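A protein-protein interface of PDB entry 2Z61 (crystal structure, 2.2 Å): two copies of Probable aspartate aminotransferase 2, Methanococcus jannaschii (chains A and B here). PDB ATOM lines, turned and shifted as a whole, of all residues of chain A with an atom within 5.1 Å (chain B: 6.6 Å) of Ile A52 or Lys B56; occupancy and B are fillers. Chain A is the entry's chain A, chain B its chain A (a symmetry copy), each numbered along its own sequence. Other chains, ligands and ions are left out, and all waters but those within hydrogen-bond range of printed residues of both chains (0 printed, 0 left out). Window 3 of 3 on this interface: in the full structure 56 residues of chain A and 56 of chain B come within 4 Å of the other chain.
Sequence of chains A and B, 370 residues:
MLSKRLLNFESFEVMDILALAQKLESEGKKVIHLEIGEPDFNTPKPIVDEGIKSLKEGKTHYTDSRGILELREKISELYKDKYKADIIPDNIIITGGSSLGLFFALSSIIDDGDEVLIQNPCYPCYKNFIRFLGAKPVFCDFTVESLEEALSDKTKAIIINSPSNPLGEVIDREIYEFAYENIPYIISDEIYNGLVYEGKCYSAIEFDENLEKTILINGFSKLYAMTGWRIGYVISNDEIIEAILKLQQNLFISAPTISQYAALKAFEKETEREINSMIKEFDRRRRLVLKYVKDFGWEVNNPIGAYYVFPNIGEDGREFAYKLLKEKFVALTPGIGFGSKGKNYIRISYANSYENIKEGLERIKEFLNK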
ATOM      1  N   VAL A  48      21.127  21.404  18.896  1.00  0.00           N
ATOM      2  CA  VAL A  48      20.827  20.145  19.574  1.00  0.00           C
ATOM      3  C   VAL A  48      19.415  20.167  20.172  1.00  0.00           C
ATOM      4  O   VAL A  48      18.640  19.217  19.989  1.00  0.00           O
ATOM      5  CB  VAL A  48      21.851  19.858  20.712  1.00  0.00           C
ATOM      6  CG1 VAL A  48      21.338  18.733  21.626  1.00  0.00           C
ATOM      7  CG2 VAL A  48      23.199  19.469  20.117  1.00  0.00           C
ATOM      8  N   ASP A  49      19.072  21.252  20.873  1.00  0.00           N
ATOM      9  CA  ASP A  49      17.744  21.358  21.494  1.00  0.00           C
ATOM     10  C   ASP A  49      16.609  21.334  20.470  1.00  0.00           C
ATOM     11  O   ASP A  49      15.562  20.742  20.709  1.00  0.00           O
ATOM     12  CB  ASP A  49      17.640  22.626  22.361  1.00  0.00           C
ATOM     13  CG  ASP A  49      18.639  22.632  23.520  1.00  0.00           C
ATOM     14  OD1 ASP A  49      19.103  21.548  23.916  1.00  0.00           O
ATOM     15  OD2 ASP A  49      18.955  23.715  24.049  1.00  0.00           O
ATOM     16  N   GLU A  50      16.820  21.972  19.326  1.00  0.00           N
ATOM     17  CA  GLU A  50      15.806  21.999  18.283  1.00  0.00           C
ATOM     18  C   GLU A  50      15.605  20.583  17.730  1.00  0.00           C
ATOM     19  O   GLU A  50      14.503  20.213  17.318  1.00  0.00           O
ATOM     20  CB  GLU A  50      16.241  22.955  17.171  1.00  0.00           C
ATOM     21  CG  GLU A  50      15.140  23.353  16.214  1.00  0.00           C
ATOM     22  CD  GLU A  50      13.883  23.795  16.946  1.00  0.00           C
ATOM     23  OE1 GLU A  50      14.017  24.419  18.022  1.00  0.00           O
ATOM     24  OE2 GLU A  50      12.770  23.527  16.441  1.00  0.00           O
ATOM     25  N   GLY A  51      16.681  19.798  17.723  1.00  0.00           N
ATOM     26  CA  GLY A  51      16.592  18.433  17.246  1.00  0.00           C
ATOM     27  C   GLY A  51      15.782  17.614  18.241  1.00  0.00           C
ATOM     28  O   GLY A  51      14.965  16.778  17.862  1.00  0.00           O
ATOM     29  N   ILE A  52      16.013  17.857  19.528  1.00  0.00           N
ATOM     30  CA  ILE A  52      15.290  17.153  20.578  1.00  0.00           C
ATOM     31  C   ILE A  52      13.802  17.495  20.498  1.00  0.00           C
ATOM     32  O   ILE A  52      12.946  16.611  20.544  1.00  0.00           O
ATOM     33  CB  ILE A  52      15.849  17.527  21.965  1.00  0.00           C
ATOM     34  CG1 ILE A  52      17.196  16.816  22.170  1.00  0.00           C
ATOM     35  CG2 ILE A  52      14.841  17.166  23.059  1.00  0.00           C
ATOM     36  CD1 ILE A  52      18.016  17.331  23.338  1.00  0.00           C
ATOM     37  N   LYS A  53      13.503  18.782  20.360  1.00  0.00           N
ATOM     38  CA  LYS A  53      12.128  19.236  20.255  1.00  0.00           C
ATOM     39  C   LYS A  53      11.420  18.641  19.038  1.00  0.00           C
ATOM     40  O   LYS A  53      10.249  18.276  19.116  1.00  0.00           O
ATOM     41  CB  LYS A  53      12.082  20.763  20.165  1.00  0.00           C
ATOM     42  CG  LYS A  53      10.684  21.323  19.951  1.00  0.00           C
ATOM     43  CD  LYS A  53      10.703  22.839  19.760  1.00  0.00           C
ATOM     44  CE  LYS A  53       9.308  23.357  19.434  1.00  0.00           C
ATOM     45  NZ  LYS A  53       9.290  24.811  19.128  1.00  0.00           N
ATOM     46  N   SER A  54      12.123  18.559  17.910  1.00  0.00           N
ATOM     47  CA  SER A  54      11.536  18.011  16.693  1.00  0.00           C
ATOM     48  C   SER A  54      11.078  16.574  16.912  1.00  0.00           C
ATOM     49  O   SER A  54       9.972  16.197  16.517  1.00  0.00           O
ATOM     50  CB  SER A  54      12.550  18.054  15.546  1.00  0.00           C
ATOM     51  OG  SER A  54      12.890  19.392  15.247  1.00  0.00           O
ATOM     52  N   LEU A  55      11.933  15.775  17.543  1.00  0.00           N
ATOM     53  CA  LEU A  55      11.609  14.383  17.825  1.00  0.00           C
ATOM     54  C   LEU A  55      10.354  14.251  18.689  1.00  0.00           C
ATOM     55  O   LEU A  55       9.508  13.389  18.446  1.00  0.00           O
ATOM     56  CB  LEU A  55      12.789  13.700  18.518  1.00  0.00           C
ATOM     57  CG  LEU A  55      13.941  13.275  17.606  1.00  0.00           C
ATOM     58  CD1 LEU A  55      15.103  12.754  18.438  1.00  0.00           C
ATOM     59  CD2 LEU A  55      13.443  12.194  16.655  1.00  0.00           C
ATOM     60  N   LYS A  56      10.239  15.114  19.696  1.00  0.00           N
ATOM     61  CA  LYS A  56       9.095  15.089  20.593  1.00  0.00           C
ATOM     62  C   LYS A  56       7.815  15.464  19.852  1.00  0.00           C
ATOM     63  O   LYS A  56       6.720  15.105  20.273  1.00  0.00           O
ATOM     64  CB  LYS A  56       9.327  16.051  21.765  1.00  0.00           C
ATOM     65  CG  LYS A  56      10.555  15.705  22.605  1.00  0.00           C
ATOM     66  CD  LYS A  56      10.930  16.830  23.556  1.00  0.00           C
ATOM     67  CE  LYS A  56       9.992  16.895  24.742  1.00  0.00           C
ATOM     68  NZ  LYS A  56      10.334  18.023  25.646  1.00  0.00           N
ATOM     69  N   GLY B  51      16.702   8.377  20.570  1.00  0.00           N
ATOM     70  CA  GLY B  51      17.239   9.409  19.706  1.00  0.00           C
ATOM     71  C   GLY B  51      17.444  10.678  20.521  1.00  0.00           C
ATOM     72  O   GLY B  51      18.440  11.381  20.365  1.00  0.00           O
ATOM     73  N   ILE B  52      16.490  10.973  21.399  1.00  0.00           N
ATOM     74  CA  ILE B  52      16.578  12.151  22.253  1.00  0.00           C
ATOM     75  C   ILE B  52      17.780  12.022  23.188  1.00  0.00           C
ATOM     76  O   ILE B  52      18.573  12.953  23.333  1.00  0.00           O
ATOM     77  CB  ILE B  52      15.282  12.325  23.070  1.00  0.00           C
ATOM     78  CG1 ILE B  52      14.176  12.857  22.146  1.00  0.00           C
ATOM     79  CG2 ILE B  52      15.527  13.254  24.261  1.00  0.00           C
ATOM     80  CD1 ILE B  52      12.774  12.775  22.721  1.00  0.00           C
ATOM     81  N   LYS B  53      17.919  10.854  23.806  1.00  0.00           N
ATOM     82  CA  LYS B  53      19.028  10.598  24.707  1.00  0.00           C
ATOM     83  C   LYS B  53      20.378  10.715  24.001  1.00  0.00           C
ATOM     84  O   LYS B  53      21.334  11.240  24.567  1.00  0.00           O
ATOM     85  CB  LYS B  53      18.900   9.201  25.317  1.00  0.00           C
ATOM     86  CG  LYS B  53      20.075   8.807  26.200  1.00  0.00           C
ATOM     87  CD  LYS B  53      19.954   7.367  26.697  1.00  0.00           C
ATOM     88  CE  LYS B  53      21.196   6.963  27.481  1.00  0.00           C
ATOM     89  NZ  LYS B  53      21.179   5.534  27.891  1.00  0.00           N
ATOM     90  N   SER B  54      20.463  10.210  22.771  1.00  0.00           N
ATOM     91  CA  SER B  54      21.708  10.268  22.015  1.00  0.00           C
ATOM     92  C   SER B  54      22.158  11.711  21.822  1.00  0.00           C
ATOM     93  O   SER B  54      23.332  12.037  22.012  1.00  0.00           O
ATOM     94  CB  SER B  54      21.534   9.599  20.649  1.00  0.00           C
ATOM     95  OG  SER B  54      21.239   8.228  20.811  1.00  0.00           O
ATOM     96  N   LEU B  55      21.220  12.572  21.440  1.00  0.00           N
ATOM     97  CA  LEU B  55      21.519  13.983  21.233  1.00  0.00           C
ATOM     98  C   LEU B  55      22.062  14.645  22.501  1.00  0.00           C
ATOM     99  O   LEU B  55      23.007  15.433  22.446  1.00  0.00           O
ATOM    100  CB  LEU B  55      20.265  14.721  20.761  1.00  0.00           C
ATOM    101  CG  LEU B  55      19.911  14.551  19.282  1.00  0.00           C
ATOM    102  CD1 LEU B  55      18.570  15.206  18.986  1.00  0.00           C
ATOM    103  CD2 LEU B  55      21.008  15.185  18.438  1.00  0.00           C
ATOM    104  N   LYS B  56      21.460  14.316  23.641  1.00  0.00           N
ATOM    105  CA  LYS B  56      21.879  14.880  24.913  1.00  0.00           C
ATOM    106  C   LYS B  56      23.284  14.413  25.279  1.00  0.00           C
ATOM    107  O   LYS B  56      23.983  15.067  26.047  1.00  0.00           O
ATOM    108  CB  LYS B  56      20.888  14.484  26.015  1.00  0.00           C
ATOM    109  CG  LYS B  56      19.464  14.975  25.761  1.00  0.00           C
ATOM    110  CD  LYS B  56      18.460  14.319  26.695  1.00  0.00           C
ATOM    111  CE  LYS B  56      18.536  14.896  28.091  1.00  0.00           C
ATOM    112  NZ  LYS B  56      17.585  14.222  29.012  1.00  0.00           N
ATOM    113  N   GLU B  57      23.707  13.285  24.719  1.00  0.00           N
ATOM    114  CA  GLU B  57      25.035  12.772  25.019  1.00  0.00           C
ATOM    115  C   GLU B  57      26.068  13.171  23.964  1.00  0.00           C
ATOM    116  O   GLU B  57      27.208  12.723  24.009  1.00  0.00           O
ATOM    117  CB  GLU B  57      24.990  11.251  25.163  1.00  0.00           C
ATOM    118  CG  GLU B  57      23.974  10.768  26.185  1.00  0.00           C
ATOM    119  CD  GLU B  57      23.985   9.259  26.351  1.00  0.00           C
ATOM    120  OE1 GLU B  57      23.938   8.538  25.330  1.00  0.00           O
ATOM    121  OE2 GLU B  57      24.036   8.792  27.507  1.00  0.00           O
ATOM    122  N   GLY B  58      25.669  14.016  23.018  1.00  0.00           N
ATOM    123  CA  GLY B  58      26.604  14.452  21.991  1.00  0.00           C
ATOM    124  C   GLY B  58      27.002  13.452  20.911  1.00  0.00           C
ATOM    125  O   GLY B  58      28.116  13.519  20.401  1.00  0.00           O
ATOM    126  N   LYS B  59      26.115  12.524  20.563  1.00  0.00           N
ATOM    127  CA  LYS B  59      26.405  11.551  19.510  1.00  0.00           C
ATOM    128  C   LYS B  59      26.172  12.263  18.178  1.00  0.00           C
ATOM    129  O   LYS B  59      25.228  11.946  17.457  1.00  0.00           O
ATOM    130  CB  LYS B  59      25.452  10.360  19.613  1.00  0.00           C
ATOM    131  CG  LYS B  59      25.532   9.603  20.923  1.00  0.00           C
ATOM    132  CD  LYS B  59      26.907   9.014  21.138  1.00  0.00           C
ATOM    133  CE  LYS B  59      26.965   8.256  22.461  1.00  0.00           C
ATOM    134  NZ  LYS B  59      25.862   7.264  22.603  1.00  0.00           N
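Of the 9 printed residues of chain B, 4 touch a printed residue of chain A.
Printed residues of chain B that touch a printed residue of chain A: Gly B51, Ile B52, Leu B55 and Lys B56.
Hydrophobic or aromatic side chains of chain B within 4 Å of the printed part of chain A: Ile B52 and Leu B55.
Of the 9 printed residues of chain A, 5 touch a printed residue of chain B.
Hydrophobic or aromatic side chains of chain A within 4 Å of the printed part of chain B: Val A48, Ile A52 and Leu A55.
Among the printed residues, no Asp or Glu carboxylate lies within 4 Å of a Lys or Arg side-chain nitrogen of the other chain.
Of the printed residues of chain B, Val A48 touches Leu B55.
Of the printed residues of chain B, Gly A51 touches Leu B55.
Ile A52 touches just these residues of chain B: Leu B55 and Lys B56.
Of chain A, only Ile A52 comes within 4 Å of Lys B56.
Gly B58 touches none of the printed residues of chain A.
The nearest residue of chain B that does not touch Ile A52 is Ile B52 (4.1 Å).
The nearest printed residue of chain A that does not touch Leu B55 is Leu A55 (4.3 Å).
Gly A51 touches Leu B55, and with the chains exchanged Leu A55 touches Gly B51.
Ile A52 touches Leu B55, and with the chains exchanged Leu A55 touches Ile B52.
Ile A52 touches Lys B56, and with the chains exchanged Lys A56 touches Ile B52.
Positions printed for both chains: 51, 52, 53, 54, 55 and 56.
Of the 7 pairs that touch across the chains among the printed residues, 6 have their exchanged pair printed and touching as well.
Val A48 touches Leu B55.
Leu B55 touches Gly A51 (CD1 to C, 3.8 Å).
CD1 of Leu B55 touches N of Ile A52 (3.7 Å).
CD1 of Ile A52 touches CG of Lys B56, at 3.7 Å.
CD1 of Leu A55 touches C of Gly B51, 3.8 Å away.
Leu A55 touches Ile B52 (CD1 to N, 3.7 Å).
CD1 of Ile B52 touches CG of Lys A56 (3.7 Å).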
